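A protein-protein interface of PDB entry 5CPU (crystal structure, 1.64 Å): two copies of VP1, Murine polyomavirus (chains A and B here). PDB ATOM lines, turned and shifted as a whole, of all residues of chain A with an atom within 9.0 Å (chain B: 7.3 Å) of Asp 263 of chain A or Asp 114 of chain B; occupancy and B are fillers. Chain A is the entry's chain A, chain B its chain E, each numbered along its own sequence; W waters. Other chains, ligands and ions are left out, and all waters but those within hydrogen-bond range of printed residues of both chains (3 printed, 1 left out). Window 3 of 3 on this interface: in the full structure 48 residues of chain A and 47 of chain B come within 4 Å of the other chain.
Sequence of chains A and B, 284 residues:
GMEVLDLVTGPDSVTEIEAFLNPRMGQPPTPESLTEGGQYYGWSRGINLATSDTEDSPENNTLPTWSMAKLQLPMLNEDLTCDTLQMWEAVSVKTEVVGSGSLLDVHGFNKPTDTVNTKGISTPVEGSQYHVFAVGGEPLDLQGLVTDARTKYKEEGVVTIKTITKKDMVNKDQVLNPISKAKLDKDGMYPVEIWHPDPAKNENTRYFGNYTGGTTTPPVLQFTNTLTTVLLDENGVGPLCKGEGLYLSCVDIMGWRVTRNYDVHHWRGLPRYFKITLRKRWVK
N of Ile 47 of chain A is in hydrogen-bond range of O of His 265 of chain A (3.0 Å).
The side-chain amino group of Lys 111 of chain A is in salt-bridge range of the side-chain carboxylate of Asp 263 of chain A, at 3.0 Å.
ND1 of His 265 of chain A sits at hydrogen-bond distance from O of Asp 263 of chain A (2.8 Å).
The backbone carbonyl oxygen of Ile 121 of chain B lies within hydrogen-bond range of the backbone NH of Thr 113 of chain B (2.9 Å).
OD1 of Asp 114 of chain B is in hydrogen-bond range of N of Val 116 of chain B, 3.1 Å away.
The side-chain amide nitrogen (ND2) of Asn 117 of chain B is in hydrogen-bond range of the side-chain carboxylate (OD2) of Asp 114 of chain B (3.0 Å).
CD1 of Leu 49 of chain A touches O of Gly 120 of chain B, 3.6 Å away.
Leu 49 of chain A touches Ile 121 of chain B.
CG2 of Thr 215 of chain A touches CG2 of Thr 113 of chain B, at 3.999 Å.
Trp 256 of chain A touches Ile 121 of chain B.
Lys 119 of chain B touches Tyr 262 of chain A.
Gly 120 of chain B touches Tyr 262 of chain A (N to O, 3.6 Å).
CB of Asp 114 of chain B touches OD2 of Asp 263 of chain A, 3.6 Å away.
O of Asp 263 of chain A touches CA of Gly 120 of chain B (3.4 Å).
His 265 of chain A touches Thr 113 of chain B (CE1 to OG1, 3.9 Å).
CG of His 265 of chain A touches CG2 of Ile 121 of chain B, 3.4 Å away.
Asp 263 of chain A touches two residues of chain B.
Asp 114 of chain B touches one residue of chain A.
No residue of chain A comes within 4 Å of Thr 115 of chain B.
Of the printed residues of chain A, Thr 113 of chain B touches Thr 215 (3.999 Å) and His 265 (3.9 Å).
Printed residues of chain B within 4 Å of Trp 256 of chain A: Ile 121 (3.6 Å).
Pro 112 of chain A touches none of the printed residues of chain B.
The nearest residue of chain B that does not touch Asp 263 of chain A is Lys 119 of chain B (4.8 Å).
The nearest residue of chain A that does not touch Asp 114 of chain B is Tyr 262 of chain A (4.9 Å).
The nearest printed residue of chain B that does not touch Trp 256 of chain A is Thr 113 of chain B (7.0 Å).
Hydrophobic or aromatic side chains of chain B that line the printed part of chain A: Ile 121.
Along chain B the printed residues that touch a printed residue of chain A span positions 113 to 121.
Among the printed residues, 10 pairs touch across the chains.
Among the printed residues, no Asp or Glu carboxylate lies within 4 Å of a Lys or Arg side-chain nitrogen of the other chain.
3 positions are printed for both chains.
Of the 10 pairs that touch across the chains among the printed residues, none has its exchanged pair printed and touching as well.
Water W3 lies within hydrogen-bond range of the side-chain hydroxyl of Thr 113 of chain B (2.7 Å) and the side-chain carboxylate of Asp 263 of chain A (2.7 Å).
Water W1 lies within hydrogen-bond range of the side-chain carboxylate of Asp 114 of chain B (2.7 Å) and the side-chain carboxylate of Asp 263 of chain A (3.0 Å).
Water W2 lies within hydrogen-bond range of O of Gly 120 of chain B (2.8 Å), N of His 265 of chain A (2.9 Å) and O of Ile 47 of chain A (2.9 Å).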
ATOM      1  N   GLY A  46      10.096  21.504  -4.245  1.00  0.00           N
ATOM      2  CA  GLY A  46       8.701  21.765  -4.619  1.00  0.00           C
ATOM      3  C   GLY A  46       7.780  21.766  -3.418  1.00  0.00           C
ATOM      4  O   GLY A  46       7.772  20.821  -2.623  1.00  0.00           O
ATOM      5  N   ILE A  47       6.997  22.822  -3.299  1.00  0.00           N
ATOM      6  CA  ILE A  47       6.123  23.004  -2.132  1.00  0.00           C
ATOM      7  C   ILE A  47       5.044  21.917  -2.107  1.00  0.00           C
ATOM      8  O   ILE A  47       4.356  21.697  -3.105  1.00  0.00           O
ATOM      9  CB  ILE A  47       5.545  24.433  -2.101  1.00  0.00           C
ATOM     10  CG1 ILE A  47       6.689  25.407  -1.781  1.00  0.00           C
ATOM     11  CG2 ILE A  47       4.416  24.540  -1.076  1.00  0.00           C
ATOM     12  CD1 ILE A  47       6.390  26.879  -2.023  1.00  0.00           C
ATOM     13  N   ASN A  48       4.978  21.206  -0.972  1.00  0.00           N
ATOM     14  CA  ASN A  48       4.041  20.106  -0.730  1.00  0.00           C
ATOM     15  C   ASN A  48       2.864  20.592   0.117  1.00  0.00           C
ATOM     16  O   ASN A  48       3.068  21.258   1.120  1.00  0.00           O
ATOM     17  CB  ASN A  48       4.751  18.843  -0.125  1.00  0.00           C
ATOM     18  CG  ASN A  48       5.195  18.987   1.358  1.00  0.00           C
ATOM     19  OD1 ASN A  48       6.237  19.582   1.682  1.00  0.00           O
ATOM     20  ND2 ASN A  48       4.443  18.347   2.255  1.00  0.00           N
ATOM     21  N   LEU A  49       1.651  20.277  -0.324  1.00  0.00           N
ATOM     22  CA  LEU A  49       0.453  20.792   0.338  1.00  0.00           C
ATOM     23  C   LEU A  49      -0.136  19.822   1.333  1.00  0.00           C
ATOM     24  O   LEU A  49      -0.035  18.605   1.163  1.00  0.00           O
ATOM     25  CB  LEU A  49      -0.612  21.158  -0.682  1.00  0.00           C
ATOM     26  CG  LEU A  49      -0.176  22.221  -1.697  1.00  0.00           C
ATOM     27  CD1 LEU A  49      -1.386  22.636  -2.508  1.00  0.00           C
ATOM     28  CD2 LEU A  49       0.461  23.432  -1.021  1.00  0.00           C
ATOM     29  N   ASN A 110       9.968  26.963 -17.268  1.00  0.00           N
ATOM     30  CA  ASN A 110       8.870  27.204 -16.323  1.00  0.00           C
ATOM     31  C   ASN A 110       7.524  27.099 -17.037  1.00  0.00           C
ATOM     32  O   ASN A 110       7.474  27.031 -18.265  1.00  0.00           O
ATOM     33  CB  ASN A 110       8.975  28.596 -15.671  1.00  0.00           C
ATOM     34  CG  ASN A 110      10.265  28.811 -14.888  1.00  0.00           C
ATOM     35  OD1 ASN A 110      11.001  27.867 -14.575  1.00  0.00           O
ATOM     36  ND2 ASN A 110      10.530  30.074 -14.541  1.00  0.00           N
ATOM     37  N   LYS A 111       6.432  27.087 -16.267  1.00  0.00           N
ATOM     38  CA  LYS A 111       5.094  27.218 -16.837  1.00  0.00           C
ATOM     39  C   LYS A 111       5.108  28.406 -17.808  1.00  0.00           C
ATOM     40  O   LYS A 111       5.509  29.503 -17.417  1.00  0.00           O
ATOM     41  CB  LYS A 111       4.085  27.480 -15.713  1.00  0.00           C
ATOM     42  CG  LYS A 111       2.636  27.447 -16.181  1.00  0.00           C
ATOM     43  CD  LYS A 111       1.683  27.680 -15.020  1.00  0.00           C
ATOM     44  CE  LYS A 111       0.251  27.450 -15.479  1.00  0.00           C
ATOM     45  NZ  LYS A 111      -0.711  27.487 -14.346  1.00  0.00           N
ATOM     46  N   PRO A 112       4.706  28.185 -19.074  1.00  0.00           N
ATOM     47  CA  PRO A 112       4.777  29.272 -20.053  1.00  0.00           C
ATOM     48  C   PRO A 112       3.599  30.230 -19.915  1.00  0.00           C
ATOM     49  O   PRO A 112       2.589  29.886 -19.298  1.00  0.00           O
ATOM     50  CB  PRO A 112       4.721  28.536 -21.390  1.00  0.00           C
ATOM     51  CG  PRO A 112       3.912  27.322 -21.107  1.00  0.00           C
ATOM     52  CD  PRO A 112       4.239  26.926 -19.688  1.00  0.00           C
ATOM     53  N   THR A 115      -0.558  29.041 -22.196  1.00  0.00           N
ATOM     54  CA  THR A 115      -0.774  27.623 -21.895  1.00  0.00           C
ATOM     55  C   THR A 115      -1.666  26.915 -22.926  1.00  0.00           C
ATOM     56  O   THR A 115      -1.826  25.695 -22.869  1.00  0.00           O
ATOM     57  CB  THR A 115      -1.289  27.394 -20.456  1.00  0.00           C
ATOM     58  OG1 THR A 115      -2.432  28.221 -20.211  1.00  0.00           O
ATOM     59  CG2 THR A 115      -0.195  27.722 -19.438  1.00  0.00           C
ATOM     60  N   THR A 215       0.135  36.128  -4.842  1.00  0.00           N
ATOM     61  CA  THR A 215       0.564  34.950  -5.611  1.00  0.00           C
ATOM     62  C   THR A 215       1.276  35.325  -6.904  1.00  0.00           C
ATOM     63  O   THR A 215       2.188  34.613  -7.331  1.00  0.00           O
ATOM     64  CB  THR A 215      -0.613  34.001  -5.941  1.00  0.00           C
ATOM     65  OG1 THR A 215      -1.562  34.676  -6.760  1.00  0.00           O
ATOM     66  CG2 THR A 215      -1.315  33.553  -4.670  1.00  0.00           C
ATOM     67  N   TRP A 256       8.174  32.908  -6.199  1.00  0.00           N
ATOM     68  CA  TRP A 256       8.304  31.516  -6.648  1.00  0.00           C
ATOM     69  C   TRP A 256       8.463  31.433  -8.147  1.00  0.00           C
ATOM     70  O   TRP A 256       7.958  32.294  -8.871  1.00  0.00           O
ATOM     71  CB  TRP A 256       7.022  30.714  -6.351  1.00  0.00           C
ATOM     72  CG  TRP A 256       6.526  30.759  -4.948  1.00  0.00           C
ATOM     73  CD1 TRP A 256       6.974  30.012  -3.898  1.00  0.00           C
ATOM     74  CD2 TRP A 256       5.479  31.593  -4.437  1.00  0.00           C
ATOM     75  NE1 TRP A 256       6.269  30.327  -2.758  1.00  0.00           N
ATOM     76  CE2 TRP A 256       5.349  31.300  -3.063  1.00  0.00           C
ATOM     77  CE3 TRP A 256       4.632  32.552  -5.013  1.00  0.00           C
ATOM     78  CZ2 TRP A 256       4.406  31.937  -2.241  1.00  0.00           C
ATOM     79  CZ3 TRP A 256       3.691  33.187  -4.195  1.00  0.00           C
ATOM     80  CH2 TRP A 256       3.588  32.877  -2.832  1.00  0.00           C
ATOM     81  N   ARG A 257       9.137  30.376  -8.609  1.00  0.00           N
ATOM     82  CA  ARG A 257       8.958  29.911  -9.986  1.00  0.00           C
ATOM     83  C   ARG A 257       7.939  28.783  -9.957  1.00  0.00           C
ATOM     84  O   ARG A 257       7.770  28.113  -8.919  1.00  0.00           O
ATOM     85  CB  ARG A 257      10.272  29.432 -10.630  1.00  0.00           C
ATOM     86  CG  ARG A 257      10.760  28.059 -10.169  1.00  0.00           C
ATOM     87  CD  ARG A 257      11.981  27.593 -10.955  1.00  0.00           C
ATOM     88  NE  ARG A 257      12.754  26.604 -10.205  1.00  0.00           N
ATOM     89  CZ  ARG A 257      12.623  25.286 -10.321  1.00  0.00           C
ATOM     90  NH1 ARG A 257      13.372  24.480  -9.579  1.00  0.00           N
ATOM     91  NH2 ARG A 257      11.751  24.768 -11.173  1.00  0.00           N
ATOM     92  N   VAL A 258       7.272  28.570 -11.088  1.00  0.00           N
ATOM     93  CA  VAL A 258       6.225  27.560 -11.208  1.00  0.00           C
ATOM     94  C   VAL A 258       6.565  26.629 -12.370  1.00  0.00           C
ATOM     95  O   VAL A 258       6.855  27.093 -13.479  1.00  0.00           O
ATOM     96  CB  VAL A 258       4.848  28.226 -11.451  1.00  0.00           C
ATOM     97  CG1 VAL A 258       3.744  27.185 -11.516  1.00  0.00           C
ATOM     98  CG2 VAL A 258       4.529  29.241 -10.358  1.00  0.00           C
ATOM     99  N   THR A 259       6.535  25.323 -12.118  1.00  0.00           N
ATOM    100  CA  THR A 259       6.919  24.356 -13.140  1.00  0.00           C
ATOM    101  C   THR A 259       5.758  24.032 -14.079  1.00  0.00           C
ATOM    102  O   THR A 259       4.618  24.448 -13.857  1.00  0.00           O
ATOM    103  CB  THR A 259       7.435  23.041 -12.516  1.00  0.00           C
ATOM    104  OG1 THR A 259       6.318  22.278 -12.037  1.00  0.00           O
ATOM    105  CG2 THR A 259       8.404  23.327 -11.376  1.00  0.00           C
ATOM    106  N   ARG A 260       6.053  23.264 -15.126  1.00  0.00           N
ATOM    107  CA  ARG A 260       5.041  22.823 -16.078  1.00  0.00           C
ATOM    108  C   ARG A 260       4.295  21.571 -15.618  1.00  0.00           C
ATOM    109  O   ARG A 260       3.440  21.060 -16.335  1.00  0.00           O
ATOM    110  CB  ARG A 260       5.692  22.545 -17.431  1.00  0.00           C
ATOM    111  CG  ARG A 260       6.237  23.795 -18.092  1.00  0.00           C
ATOM    112  CD  ARG A 260       6.800  23.434 -19.454  1.00  0.00           C
ATOM    113  NE  ARG A 260       7.287  24.602 -20.190  1.00  0.00           N
ATOM    114  CZ  ARG A 260       7.396  24.632 -21.520  1.00  0.00           C
ATOM    115  NH1 ARG A 260       7.065  23.563 -22.238  1.00  0.00           N
ATOM    116  NH2 ARG A 260       7.849  25.720 -22.135  1.00  0.00           N
ATOM    117  N   ASN A 261       4.634  21.071 -14.433  1.00  0.00           N
ATOM    118  CA  ASN A 261       3.991  19.855 -13.933  1.00  0.00           C
ATOM    119  C   ASN A 261       3.229  20.124 -12.645  1.00  0.00           C
ATOM    120  O   ASN A 261       3.821  20.355 -11.591  1.00  0.00           O
ATOM    121  CB  ASN A 261       5.005  18.723 -13.773  1.00  0.00           C
ATOM    122  CG  ASN A 261       5.531  18.222 -15.107  1.00  0.00           C
ATOM    123  OD1 ASN A 261       6.730  18.267 -15.360  1.00  0.00           O
ATOM    124  ND2 ASN A 261       4.632  17.745 -15.972  1.00  0.00           N
ATOM    125  N   TYR A 262       1.904  20.146 -12.774  1.00  0.00           N
ATOM    126  CA  TYR A 262       0.996  20.436 -11.661  1.00  0.00           C
ATOM    127  C   TYR A 262       1.339  21.692 -10.872  1.00  0.00           C
ATOM    128  O   TYR A 262       1.189  21.733  -9.650  1.00  0.00           O
ATOM    129  CB  TYR A 262       0.878  19.225 -10.728  1.00  0.00           C
ATOM    130  CG  TYR A 262       0.091  18.086 -11.338  1.00  0.00           C
ATOM    131  CD1 TYR A 262      -1.168  18.308 -11.910  1.00  0.00           C
ATOM    132  CD2 TYR A 262       0.598  16.789 -11.339  1.00  0.00           C
ATOM    133  CE1 TYR A 262      -1.895  17.270 -12.472  1.00  0.00           C
ATOM    134  CE2 TYR A 262      -0.122  15.742 -11.898  1.00  0.00           C
ATOM    135  CZ  TYR A 262      -1.367  15.989 -12.462  1.00  0.00           C
ATOM    136  OH  TYR A 262      -2.093  14.960 -13.019  1.00  0.00           O
ATOM    137  N   ASP A 263       1.816  22.725 -11.574  1.00  0.00           N
ATOM    138  CA  ASP A 263       2.033  24.029 -10.974  1.00  0.00           C
ATOM    139  C   ASP A 263       2.915  23.971  -9.714  1.00  0.00           C
ATOM    140  O   ASP A 263       2.668  24.703  -8.765  1.00  0.00           O
ATOM    141  CB  ASP A 263       0.684  24.683 -10.600  1.00  0.00           C
ATOM    142  CG  ASP A 263      -0.043  25.311 -11.785  1.00  0.00           C
ATOM    143  OD1 ASP A 263       0.274  25.015 -12.954  1.00  0.00           O
ATOM    144  OD2 ASP A 263      -0.980  26.107 -11.534  1.00  0.00           O
ATOM    145  N   VAL A 264       3.935  23.111  -9.698  1.00  0.00           N
ATOM    146  CA  VAL A 264       4.816  23.050  -8.524  1.00  0.00           C
ATOM    147  C   VAL A 264       5.561  24.366  -8.353  1.00  0.00           C
ATOM    148  O   VAL A 264       6.165  24.881  -9.304  1.00  0.00           O
ATOM    149  CB  VAL A 264       5.789  21.845  -8.583  1.00  0.00           C
ATOM    150  CG1 VAL A 264       6.775  21.891  -7.430  1.00  0.00           C
ATOM    151  CG2 VAL A 264       5.010  20.533  -8.533  1.00  0.00           C
ATOM    152  N   HIS A 265       5.474  24.934  -7.153  1.00  0.00           N
ATOM    153  CA  HIS A 265       6.179  26.173  -6.834  1.00  0.00           C
ATOM    154  C   HIS A 265       7.496  25.906  -6.113  1.00  0.00           C
ATOM    155  O   HIS A 265       7.579  25.037  -5.234  1.00  0.00           O
ATOM    156  CB  HIS A 265       5.334  27.080  -5.938  1.00  0.00           C
ATOM    157  CG  HIS A 265       4.159  27.718  -6.618  1.00  0.00           C
ATOM    158  ND1 HIS A 265       3.253  27.014  -7.385  1.00  0.00           N
ATOM    159  CD2 HIS A 265       3.702  28.994  -6.575  1.00  0.00           C
ATOM    160  CE1 HIS A 265       2.300  27.832  -7.807  1.00  0.00           C
ATOM    161  NE2 HIS A 265       2.550  29.040  -7.328  1.00  0.00           N
ATOM    162  N   HIS A 266       8.505  26.701  -6.468  1.00  0.00           N
ATOM    163  CA  HIS A 266       9.811  26.694  -5.803  1.00  0.00           C
ATOM    164  C   HIS A 266      10.132  28.117  -5.386  1.00  0.00           C
ATOM    165  O   HIS A 266      10.170  29.024  -6.231  1.00  0.00           O
ATOM    166  CB  HIS A 266      10.923  26.209  -6.742  1.00  0.00           C
ATOM    167  CG  HIS A 266      10.778  24.786  -7.175  1.00  0.00           C
ATOM    168  ND1 HIS A 266      11.486  23.760  -6.586  1.00  0.00           N
ATOM    169  CD2 HIS A 266      10.037  24.218  -8.157  1.00  0.00           C
ATOM    170  CE1 HIS A 266      11.172  22.621  -7.170  1.00  0.00           C
ATOM    171  NE2 HIS A 266      10.293  22.865  -8.127  1.00  0.00           N
ATOM    172  N   LYS B 111      -7.850  27.205  -0.158  1.00  0.00           N
ATOM    173  CA  LYS B 111      -8.139  27.131  -1.584  1.00  0.00           C
ATOM    174  C   LYS B 111      -6.805  27.153  -2.340  1.00  0.00           C
ATOM    175  O   LYS B 111      -6.001  28.057  -2.114  1.00  0.00           O
ATOM    176  CB  LYS B 111      -8.974  28.335  -1.996  1.00  0.00           C
ATOM    177  CG  LYS B 111      -9.460  28.270  -3.434  1.00  0.00           C
ATOM    178  CD  LYS B 111     -10.369  29.464  -3.707  1.00  0.00           C
ATOM    179  CE  LYS B 111     -10.837  29.473  -5.150  1.00  0.00           C
ATOM    180  NZ  LYS B 111     -11.948  30.460  -5.285  1.00  0.00           N
ATOM    181  N   PRO B 112      -6.559  26.160  -3.211  1.00  0.00           N
ATOM    182  CA  PRO B 112      -5.256  26.105  -3.874  1.00  0.00           C
ATOM    183  C   PRO B 112      -5.217  27.005  -5.107  1.00  0.00           C
ATOM    184  O   PRO B 112      -6.273  27.400  -5.630  1.00  0.00           O
ATOM    185  CB  PRO B 112      -5.135  24.633  -4.267  1.00  0.00           C
ATOM    186  CG  PRO B 112      -6.549  24.213  -4.525  1.00  0.00           C
ATOM    187  CD  PRO B 112      -7.363  24.950  -3.488  1.00  0.00           C
ATOM    188  N   THR B 113      -4.014  27.325  -5.573  1.00  0.00           N
ATOM    189  CA  THR B 113      -3.894  28.185  -6.757  1.00  0.00           C
ATOM    190  C   THR B 113      -4.306  27.504  -8.064  1.00  0.00           C
ATOM    191  O   THR B 113      -4.707  28.187  -9.015  1.00  0.00           O
ATOM    192  CB  THR B 113      -2.494  28.819  -6.871  1.00  0.00           C
ATOM    193  OG1 THR B 113      -1.499  27.791  -6.846  1.00  0.00           O
ATOM    194  CG2 THR B 113      -2.265  29.815  -5.726  1.00  0.00           C
ATOM    195  N   ASP B 114      -4.203  26.173  -8.122  1.00  0.00           N
ATOM    196  CA  ASP B 114      -4.731  25.392  -9.247  1.00  0.00           C
ATOM    197  C   ASP B 114      -5.941  24.610  -8.734  1.00  0.00           C
ATOM    198  O   ASP B 114      -5.784  23.529  -8.158  1.00  0.00           O
ATOM    199  CB  ASP B 114      -3.657  24.445  -9.806  1.00  0.00           C
ATOM    200  CG  ASP B 114      -4.199  23.471 -10.863  1.00  0.00           C
ATOM    201  OD1 ASP B 114      -5.407  23.515 -11.198  1.00  0.00           O
ATOM    202  OD2 ASP B 114      -3.401  22.647 -11.350  1.00  0.00           O
ATOM    203  N   THR B 115      -7.136  25.168  -8.925  1.00  0.00           N
ATOM    204  CA  THR B 115      -8.350  24.531  -8.396  1.00  0.00           C
ATOM    205  C   THR B 115      -8.850  23.406  -9.286  1.00  0.00           C
ATOM    206  O   THR B 115      -9.601  22.544  -8.833  1.00  0.00           O
ATOM    207  CB  THR B 115      -9.507  25.528  -8.189  1.00  0.00           C
ATOM    208  OG1 THR B 115      -9.819  26.164  -9.432  1.00  0.00           O
ATOM    209  CG2 THR B 115      -9.135  26.584  -7.148  1.00  0.00           C
ATOM    210  N   VAL B 116      -8.447  23.403 -10.558  1.00  0.00           N
ATOM    211  CA  VAL B 116      -8.814  22.310 -11.459  1.00  0.00           C
ATOM    212  C   VAL B 116      -8.255  20.984 -10.944  1.00  0.00           C
ATOM    213  O   VAL B 116      -8.989  20.002 -10.796  1.00  0.00           O
ATOM    214  CB  VAL B 116      -8.322  22.576 -12.903  1.00  0.00           C
ATOM    215  CG1 VAL B 116      -8.500  21.347 -13.790  1.00  0.00           C
ATOM    216  CG2 VAL B 116      -9.025  23.793 -13.477  1.00  0.00           C
ATOM    217  N   ASN B 117      -6.958  20.971 -10.634  1.00  0.00           N
ATOM    218  CA  ASN B 117      -6.265  19.739 -10.261  1.00  0.00           C
ATOM    219  C   ASN B 117      -5.981  19.602  -8.769  1.00  0.00           C
ATOM    220  O   ASN B 117      -5.486  18.543  -8.334  1.00  0.00           O
ATOM    221  CB  ASN B 117      -4.959  19.612 -11.050  1.00  0.00           C
ATOM    222  CG  ASN B 117      -5.185  19.663 -12.543  1.00  0.00           C
ATOM    223  OD1 ASN B 117      -5.779  18.753 -13.118  1.00  0.00           O
ATOM    224  ND2 ASN B 117      -4.743  20.746 -13.177  1.00  0.00           N
ATOM    225  N   THR B 118      -6.309  20.652  -8.009  1.00  0.00           N
ATOM    226  CA  THR B 118      -6.036  20.738  -6.564  1.00  0.00           C
ATOM    227  C   THR B 118      -4.524  20.661  -6.374  1.00  0.00           C
ATOM    228  O   THR B 118      -3.993  19.735  -5.746  1.00  0.00           O
ATOM    229  CB  THR B 118      -6.771  19.629  -5.763  1.00  0.00           C
ATOM    230  OG1 THR B 118      -8.146  19.584  -6.174  1.00  0.00           O
ATOM    231  CG2 THR B 118      -6.707  19.921  -4.266  1.00  0.00           C
ATOM    232  N   LYS B 119      -3.843  21.636  -6.968  1.00  0.00           N
ATOM    233  CA  LYS B 119      -2.385  21.667  -7.017  1.00  0.00           C
ATOM    234  C   LYS B 119      -1.928  23.118  -6.853  1.00  0.00           C
ATOM    235  O   LYS B 119      -2.734  24.019  -6.593  1.00  0.00           O
ATOM    236  CB  LYS B 119      -1.871  21.079  -8.345  1.00  0.00           C
ATOM    237  CG  LYS B 119      -2.188  19.608  -8.587  1.00  0.00           C
ATOM    238  CD  LYS B 119      -1.407  18.685  -7.664  1.00  0.00           C
ATOM    239  CE  LYS B 119      -1.861  17.250  -7.863  1.00  0.00           C
ATOM    240  NZ  LYS B 119      -1.022  16.306  -7.071  1.00  0.00           N
ATOM    241  N   GLY B 120      -0.625  23.354  -6.995  1.00  0.00           N
ATOM    242  CA  GLY B 120      -0.087  24.696  -6.816  1.00  0.00           C
ATOM    243  C   GLY B 120       0.341  24.945  -5.379  1.00  0.00           C
ATOM    244  O   GLY B 120       1.023  24.102  -4.769  1.00  0.00           O
ATOM    245  N   ILE B 121      -0.050  26.095  -4.849  1.00  0.00           N
ATOM    246  CA  ILE B 121       0.168  26.392  -3.442  1.00  0.00           C
ATOM    247  C   ILE B 121      -1.142  26.695  -2.740  1.00  0.00           C
ATOM    248  O   ILE B 121      -2.158  26.992  -3.375  1.00  0.00           O
ATOM    249  CB  ILE B 121       1.175  27.550  -3.222  1.00  0.00           C
ATOM    250  CG1 ILE B 121       0.720  28.830  -3.945  1.00  0.00           C
ATOM    251  CG2 ILE B 121       2.569  27.089  -3.636  1.00  0.00           C
ATOM    252  CD1 ILE B 121       1.478  30.085  -3.545  1.00  0.00           C
ATOM    253  N   THR B 123      -3.367  29.168  -1.145  1.00  0.00           N
ATOM    254  CA  THR B 123      -3.432  30.621  -1.399  1.00  0.00           C
ATOM    255  C   THR B 123      -3.138  31.380  -0.118  1.00  0.00           C
ATOM    256  O   THR B 123      -3.781  31.135   0.910  1.00  0.00           O
ATOM    257  CB  THR B 123      -4.799  31.053  -1.957  1.00  0.00           C
ATOM    258  OG1 THR B 123      -5.073  30.330  -3.162  1.00  0.00           O
ATOM    259  CG2 THR B 123      -4.790  32.564  -2.270  1.00  0.00           C
HETATM  260  O   HOH W   1      -1.339  22.458 -13.135  1.00  0.00           O
HETATM  261  O   HOH W   2       3.762  23.690  -5.149  1.00  0.00           O
HETATM  262  O   HOH W   3      -0.597  27.726  -9.347  1.00  0.00           O
